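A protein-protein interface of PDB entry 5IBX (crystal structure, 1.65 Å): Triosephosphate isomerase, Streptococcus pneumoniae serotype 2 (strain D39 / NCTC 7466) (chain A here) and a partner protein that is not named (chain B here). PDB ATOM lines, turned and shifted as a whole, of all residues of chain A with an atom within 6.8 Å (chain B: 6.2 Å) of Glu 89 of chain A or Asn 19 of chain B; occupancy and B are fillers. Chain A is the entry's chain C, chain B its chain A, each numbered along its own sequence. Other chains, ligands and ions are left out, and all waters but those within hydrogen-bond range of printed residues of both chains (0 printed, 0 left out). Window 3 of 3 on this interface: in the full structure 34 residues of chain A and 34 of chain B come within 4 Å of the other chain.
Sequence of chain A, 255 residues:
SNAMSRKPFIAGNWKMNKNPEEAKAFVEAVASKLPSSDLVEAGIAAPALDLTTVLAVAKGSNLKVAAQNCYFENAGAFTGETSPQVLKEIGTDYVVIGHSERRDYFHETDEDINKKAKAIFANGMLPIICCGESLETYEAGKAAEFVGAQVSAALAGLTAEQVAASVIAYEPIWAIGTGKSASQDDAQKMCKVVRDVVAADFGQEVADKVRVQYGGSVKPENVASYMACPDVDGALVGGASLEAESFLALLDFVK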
ATOM      1  N   SER A  83      -0.998 -14.607  -7.939  1.00  0.00           N
ATOM      2  CA  SER A  83      -1.303 -13.190  -8.204  1.00  0.00           C
ATOM      3  C   SER A  83      -2.043 -12.953  -9.524  1.00  0.00           C
ATOM      4  O   SER A  83      -1.640 -13.502 -10.540  1.00  0.00           O
ATOM      5  CB  SER A  83      -0.020 -12.396  -8.246  1.00  0.00           C
ATOM      6  OG  SER A  83      -0.239 -11.114  -8.816  1.00  0.00           O
ATOM      7  N   PRO A  84      -3.156 -12.164  -9.493  1.00  0.00           N
ATOM      8  CA  PRO A  84      -3.870 -11.773 -10.722  1.00  0.00           C
ATOM      9  C   PRO A  84      -3.051 -10.845 -11.613  1.00  0.00           C
ATOM     10  O   PRO A  84      -3.244 -10.830 -12.834  1.00  0.00           O
ATOM     11  CB  PRO A  84      -5.115 -11.032 -10.201  1.00  0.00           C
ATOM     12  CG  PRO A  84      -4.745 -10.544  -8.851  1.00  0.00           C
ATOM     13  CD  PRO A  84      -3.818 -11.621  -8.292  1.00  0.00           C
ATOM     14  N   GLN A  85      -2.122 -10.106 -10.999  1.00  0.00           N
ATOM     15  CA  GLN A  85      -1.244  -9.235 -11.758  1.00  0.00           C
ATOM     16  C   GLN A  85      -0.306 -10.098 -12.575  1.00  0.00           C
ATOM     17  O   GLN A  85      -0.131  -9.841 -13.762  1.00  0.00           O
ATOM     18  CB  GLN A  85      -0.481  -8.280 -10.846  1.00  0.00           C
ATOM     19  CG  GLN A  85       0.354  -7.253 -11.592  1.00  0.00           C
ATOM     20  CD  GLN A  85       1.125  -6.363 -10.650  1.00  0.00           C
ATOM     21  OE1 GLN A  85       1.635  -6.810  -9.615  1.00  0.00           O
ATOM     22  NE2 GLN A  85       1.221  -5.101 -11.006  1.00  0.00           N
ATOM     23  N   VAL A  86       0.301 -11.108 -11.960  1.00  0.00           N
ATOM     24  CA  VAL A  86       1.167 -12.022 -12.720  1.00  0.00           C
ATOM     25  C   VAL A  86       0.331 -12.790 -13.745  1.00  0.00           C
ATOM     26  O   VAL A  86       0.782 -13.001 -14.833  1.00  0.00           O
ATOM     27  CB  VAL A  86       1.914 -12.993 -11.801  1.00  0.00           C
ATOM     28  CG1 VAL A  86       2.805 -13.915 -12.614  1.00  0.00           C
ATOM     29  CG2 VAL A  86       2.724 -12.215 -10.770  1.00  0.00           C
ATOM     30  N   LEU A  87      -0.882 -13.219 -13.379  1.00  0.00           N
ATOM     31  CA  LEU A  87      -1.731 -13.930 -14.386  1.00  0.00           C
ATOM     32  C   LEU A  87      -1.909 -13.069 -15.650  1.00  0.00           C
ATOM     33  O   LEU A  87      -1.801 -13.559 -16.787  1.00  0.00           O
ATOM     34  CB  LEU A  87      -3.067 -14.316 -13.781  1.00  0.00           C
ATOM     35  CG  LEU A  87      -3.007 -15.474 -12.764  1.00  0.00           C
ATOM     36  CD1 LEU A  87      -4.344 -15.689 -12.082  1.00  0.00           C
ATOM     37  CD2 LEU A  87      -2.533 -16.766 -13.398  1.00  0.00           C
ATOM     38  N   LYS A  88      -2.170 -11.774 -15.478  1.00  0.00           N
ATOM     39  CA  LYS A  88      -2.290 -10.884 -16.653  1.00  0.00           C
ATOM     40  C   LYS A  88      -0.946 -10.780 -17.374  1.00  0.00           C
ATOM     41  O   LYS A  88      -0.876 -10.909 -18.598  1.00  0.00           O
ATOM     42  CB  LYS A  88      -2.793  -9.510 -16.254  1.00  0.00           C
ATOM     43  CG  LYS A  88      -2.774  -8.486 -17.386  1.00  0.00           C
ATOM     44  CD  LYS A  88      -3.720  -8.814 -18.503  1.00  0.00           C
ATOM     45  CE  LYS A  88      -3.857  -7.640 -19.470  1.00  0.00           C
ATOM     46  NZ  LYS A  88      -2.599  -7.247 -20.158  1.00  0.00           N
ATOM     47  N   GLU A  89       0.121 -10.544 -16.614  1.00  0.00           N
ATOM     48  CA  GLU A  89       1.461 -10.412 -17.196  1.00  0.00           C
ATOM     49  C   GLU A  89       1.886 -11.577 -18.121  1.00  0.00           C
ATOM     50  O   GLU A  89       2.496 -11.362 -19.183  1.00  0.00           O
ATOM     51  CB  GLU A  89       2.481 -10.136 -16.081  1.00  0.00           C
ATOM     52  CG  GLU A  89       2.304  -8.734 -15.483  1.00  0.00           C
ATOM     53  CD  GLU A  89       3.112  -8.456 -14.218  1.00  0.00           C
ATOM     54  OE1 GLU A  89       3.739  -9.403 -13.699  1.00  0.00           O
ATOM     55  OE2 GLU A  89       3.156  -7.275 -13.739  1.00  0.00           O
ATOM     56  N   ILE A  90       1.507 -12.790 -17.765  1.00  0.00           N
ATOM     57  CA  ILE A  90       1.849 -13.955 -18.590  1.00  0.00           C
ATOM     58  C   ILE A  90       0.899 -14.165 -19.764  1.00  0.00           C
ATOM     59  O   ILE A  90       1.162 -15.018 -20.617  1.00  0.00           O
ATOM     60  CB  ILE A  90       1.978 -15.257 -17.729  1.00  0.00           C
ATOM     61  CG1 ILE A  90       0.668 -15.659 -17.048  1.00  0.00           C
ATOM     62  CG2 ILE A  90       3.079 -15.080 -16.688  1.00  0.00           C
ATOM     63  CD1 ILE A  90       0.722 -16.976 -16.282  1.00  0.00           C
ATOM     64  N   GLY A  91      -0.232 -13.457 -19.763  1.00  0.00           N
ATOM     65  CA  GLY A  91      -1.230 -13.498 -20.837  1.00  0.00           C
ATOM     66  C   GLY A  91      -2.539 -14.248 -20.602  1.00  0.00           C
ATOM     67  O   GLY A  91      -3.222 -14.569 -21.560  1.00  0.00           O
ATOM     68  N   THR A  92      -2.889 -14.537 -19.348  1.00  0.00           N
ATOM     69  CA  THR A  92      -4.106 -15.279 -19.062  1.00  0.00           C
ATOM     70  C   THR A  92      -5.372 -14.525 -19.490  1.00  0.00           C
ATOM     71  O   THR A  92      -5.458 -13.299 -19.350  1.00  0.00           O
ATOM     72  CB  THR A  92      -4.146 -15.609 -17.543  1.00  0.00           C
ATOM     73  OG1 THR A  92      -2.878 -16.147 -17.149  1.00  0.00           O
ATOM     74  CG2 THR A  92      -5.172 -16.593 -17.220  1.00  0.00           C
ATOM     75  N   ASN A 123      -7.074  -5.938 -13.130  1.00  0.00           N
ATOM     76  CA  ASN A 123      -5.928  -6.486 -13.896  1.00  0.00           C
ATOM     77  C   ASN A 123      -6.204  -6.846 -15.371  1.00  0.00           C
ATOM     78  O   ASN A 123      -5.398  -7.547 -15.992  1.00  0.00           O
ATOM     79  CB  ASN A 123      -5.316  -7.688 -13.145  1.00  0.00           C
ATOM     80  CG  ASN A 123      -4.497  -7.250 -11.951  1.00  0.00           C
ATOM     81  OD1 ASN A 123      -3.355  -6.789 -12.097  1.00  0.00           O
ATOM     82  ND2 ASN A 123      -5.076  -7.361 -10.769  1.00  0.00           N
ATOM     83  N   MET A 125      -8.497  -8.847 -16.966  1.00  0.00           N
ATOM     84  CA  MET A 125      -8.919 -10.192 -17.343  1.00  0.00           C
ATOM     85  C   MET A 125     -10.410 -10.288 -17.080  1.00  0.00           C
ATOM     86  O   MET A 125     -11.027  -9.331 -16.607  1.00  0.00           O
ATOM     87  CB  MET A 125      -8.134 -11.259 -16.564  1.00  0.00           C
ATOM     88  CG  MET A 125      -6.617 -11.248 -16.818  1.00  0.00           C
ATOM     89  SD  MET A 125      -5.715 -12.420 -15.810  1.00  0.00           S
ATOM     90  CE  MET A 125      -6.165 -11.890 -14.171  1.00  0.00           C
ATOM     91  N   TRP B  14       9.924 -15.901  -1.273  1.00  0.00           N
ATOM     92  CA  TRP B  14       9.485 -14.700  -2.021  1.00  0.00           C
ATOM     93  C   TRP B  14       8.040 -14.307  -1.732  1.00  0.00           C
ATOM     94  O   TRP B  14       7.631 -13.200  -2.046  1.00  0.00           O
ATOM     95  CB  TRP B  14       9.569 -14.901  -3.537  1.00  0.00           C
ATOM     96  CG  TRP B  14      10.935 -14.899  -4.121  1.00  0.00           C
ATOM     97  CD1 TRP B  14      12.039 -14.398  -3.569  1.00  0.00           C
ATOM     98  CD2 TRP B  14      11.292 -15.318  -5.449  1.00  0.00           C
ATOM     99  NE1 TRP B  14      13.109 -14.537  -4.445  1.00  0.00           N
ATOM    100  CE2 TRP B  14      12.656 -15.076  -5.610  1.00  0.00           C
ATOM    101  CE3 TRP B  14      10.578 -15.872  -6.515  1.00  0.00           C
ATOM    102  CZ2 TRP B  14      13.324 -15.399  -6.771  1.00  0.00           C
ATOM    103  CZ3 TRP B  14      11.236 -16.173  -7.671  1.00  0.00           C
ATOM    104  CH2 TRP B  14      12.599 -15.955  -7.787  1.00  0.00           C
ATOM    105  N   ASN B  17       5.179 -12.640  -4.792  1.00  0.00           N
ATOM    106  CA  ASN B  17       5.946 -11.638  -5.532  1.00  0.00           C
ATOM    107  C   ASN B  17       6.661 -12.304  -6.682  1.00  0.00           C
ATOM    108  O   ASN B  17       7.050 -13.462  -6.571  1.00  0.00           O
ATOM    109  CB  ASN B  17       6.976 -10.948  -4.629  1.00  0.00           C
ATOM    110  CG  ASN B  17       6.330 -10.154  -3.524  1.00  0.00           C
ATOM    111  OD1 ASN B  17       5.900  -9.032  -3.726  1.00  0.00           O
ATOM    112  ND2 ASN B  17       6.197 -10.763  -2.359  1.00  0.00           N
ATOM    113  N   LYS B  18       6.773 -11.553  -7.783  1.00  0.00           N
ATOM    114  CA  LYS B  18       7.493 -11.880  -9.019  1.00  0.00           C
ATOM    115  C   LYS B  18       6.740 -12.690 -10.072  1.00  0.00           C
ATOM    116  O   LYS B  18       6.092 -13.679  -9.764  1.00  0.00           O
ATOM    117  CB  LYS B  18       8.838 -12.565  -8.767  1.00  0.00           C
ATOM    118  CG  LYS B  18       9.791 -11.761  -7.920  1.00  0.00           C
ATOM    119  CD  LYS B  18      11.147 -12.451  -7.907  1.00  0.00           C
ATOM    120  CE  LYS B  18      12.034 -11.908  -6.804  1.00  0.00           C
ATOM    121  NZ  LYS B  18      12.353 -10.469  -6.942  1.00  0.00           N
ATOM    122  N   ASN B  19       6.856 -12.237 -11.313  1.00  0.00           N
ATOM    123  CA  ASN B  19       6.392 -12.976 -12.479  1.00  0.00           C
ATOM    124  C   ASN B  19       7.541 -13.892 -12.987  1.00  0.00           C
ATOM    125  O   ASN B  19       8.661 -13.831 -12.475  1.00  0.00           O
ATOM    126  CB  ASN B  19       5.861 -12.016 -13.558  1.00  0.00           C
ATOM    127  CG  ASN B  19       6.919 -11.154 -14.200  1.00  0.00           C
ATOM    128  OD1 ASN B  19       8.090 -11.538 -14.342  1.00  0.00           O
ATOM    129  ND2 ASN B  19       6.480 -10.005 -14.687  1.00  0.00           N
ATOM    130  N   PRO B  20       7.280 -14.739 -13.994  1.00  0.00           N
ATOM    131  CA  PRO B  20       8.368 -15.611 -14.424  1.00  0.00           C
ATOM    132  C   PRO B  20       9.638 -14.871 -14.929  1.00  0.00           C
ATOM    133  O   PRO B  20      10.763 -15.307 -14.638  1.00  0.00           O
ATOM    134  CB  PRO B  20       7.734 -16.411 -15.562  1.00  0.00           C
ATOM    135  CG  PRO B  20       6.318 -16.395 -15.304  1.00  0.00           C
ATOM    136  CD  PRO B  20       5.986 -15.150 -14.563  1.00  0.00           C
ATOM    137  N   GLU B  21       9.463 -13.779 -15.678  1.00  0.00           N
ATOM    138  CA  GLU B  21      10.619 -13.029 -16.173  1.00  0.00           C
ATOM    139  C   GLU B  21      11.443 -12.460 -15.024  1.00  0.00           C
ATOM    140  O   GLU B  21      12.683 -12.529 -15.041  1.00  0.00           O
ATOM    141  CB  GLU B  21      10.187 -11.940 -17.168  1.00  0.00           C
ATOM    142  CG  GLU B  21       9.776 -12.518 -18.516  1.00  0.00           C
ATOM    143  CD  GLU B  21      10.880 -13.379 -19.125  1.00  0.00           C
ATOM    144  OE1 GLU B  21      10.638 -14.568 -19.412  1.00  0.00           O
ATOM    145  OE2 GLU B  21      12.014 -12.897 -19.239  1.00  0.00           O
ATOM    146  N   GLU B  22      10.764 -11.931 -14.008  1.00  0.00           N
ATOM    147  CA  GLU B  22      11.458 -11.384 -12.826  1.00  0.00           C
ATOM    148  C   GLU B  22      12.163 -12.488 -12.066  1.00  0.00           C
ATOM    149  O   GLU B  22      13.286 -12.301 -11.575  1.00  0.00           O
ATOM    150  CB  GLU B  22      10.471 -10.663 -11.915  1.00  0.00           C
ATOM    151  CG  GLU B  22       9.855  -9.429 -12.582  1.00  0.00           C
ATOM    152  CD  GLU B  22       8.687  -8.856 -11.792  1.00  0.00           C
ATOM    153  OE1 GLU B  22       7.779  -9.610 -11.413  1.00  0.00           O
ATOM    154  OE2 GLU B  22       8.694  -7.639 -11.545  1.00  0.00           O
ATOM    155  N   ALA B  23      11.519 -13.651 -12.000  1.00  0.00           N
ATOM    156  CA  ALA B  23      12.076 -14.807 -11.292  1.00  0.00           C
ATOM    157  C   ALA B  23      13.316 -15.331 -12.020  1.00  0.00           C
ATOM    158  O   ALA B  23      14.350 -15.646 -11.414  1.00  0.00           O
ATOM    159  CB  ALA B  23      11.018 -15.893 -11.157  1.00  0.00           C
ATOM    160  N   LYS B  24      13.214 -15.352 -13.333  1.00  0.00           N
ATOM    161  CA  LYS B  24      14.293 -15.762 -14.187  1.00  0.00           C
ATOM    162  C   LYS B  24      15.493 -14.868 -14.001  1.00  0.00           C
ATOM    163  O   LYS B  24      16.621 -15.345 -13.851  1.00  0.00           O
ATOM    164  CB  LYS B  24      13.832 -15.685 -15.647  1.00  0.00           C
ATOM    165  CG  LYS B  24      14.831 -16.233 -16.649  1.00  0.00           C
ATOM    166  CD  LYS B  24      14.393 -16.058 -18.098  1.00  0.00           C
ATOM    167  CE  LYS B  24      13.037 -16.674 -18.385  1.00  0.00           C
ATOM    168  NZ  LYS B  24      12.793 -16.778 -19.858  1.00  0.00           N
ATOM    169  N   ASP B  50       5.699 -19.424 -11.334  1.00  0.00           N
ATOM    170  CA  ASP B  50       7.097 -19.205 -11.674  1.00  0.00           C
ATOM    171  C   ASP B  50       7.995 -20.420 -11.592  1.00  0.00           C
ATOM    172  O   ASP B  50       9.137 -20.353 -12.038  1.00  0.00           O
ATOM    173  CB  ASP B  50       7.694 -18.165 -10.696  1.00  0.00           C
ATOM    174  CG  ASP B  50       6.963 -16.826 -10.689  1.00  0.00           C
ATOM    175  OD1 ASP B  50       6.295 -16.502 -11.669  1.00  0.00           O
ATOM    176  OD2 ASP B  50       7.155 -16.042  -9.705  1.00  0.00           O
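The side-chain amide oxygen (OD1) of Asn 19 of chain B lies within hydrogen-bond range of the backbone NH (N) of Glu 21 of chain B (2.9 Å).
The side-chain hydroxyl (OG) of Ser 83 of chain A sits at hydrogen-bond distance from the backbone NH (N) of Val 86 of chain A, at 3.2 Å.
N of Glu 22 of chain B lies within hydrogen-bond range of OD1 of Asn 19 of chain B, 2.7 Å away.
The backbone carbonyl oxygen (O) of Lys 18 of chain B lies close to the side-chain carboxylate (OD2) of Asp 50 of chain B (2.6 Å).
Of the printed residues of chain B, Val 86 of chain A touches Lys 18 (3.8 Å), Asn 19 (3.7 Å) and Pro 20 (3.9 Å).
Of chain B, only Asn 19 comes within 4 Å of Glu 89 of chain A.
Printed residues of chain B within 4 Å of Ile 90 of chain A: Pro 20.
Printed residues of chain A within 4 Å of Lys 18 of chain B: Val 86.
Of the printed residues of chain A, Pro 20 of chain B touches Val 86 and Ile 90.
Lys 24 of chain B touches none of the printed residues of chain A.
The nearest residue of chain A that does not touch Asn 19 of chain B is Ile 90 of chain A (5.2 Å).
Hydrophobic or aromatic side chains of chain B that line the printed part of chain A: Pro 20.
Printed residues of chain A that touch a printed residue of chain B: Val 86, Glu 89 and Ile 90.
Among the printed residues, no Asp or Glu carboxylate lies within 4 Å of a Lys or Arg side-chain nitrogen of the other chain.
Val 86 of chain A touches Lys 18 of chain B.
Val 86 of chain A touches Asn 19 of chain B.
Val 86 of chain A touches Pro 20 of chain B (CG1 to CD, 3.9 Å).
Ile 90 of chain A touches Pro 20 of chain B.
The side-chain amide nitrogen of Asn 19 of chain B lies within hydrogen-bond range of the side-chain carboxylate of Glu 89 of chain A, at 3.0 Å.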
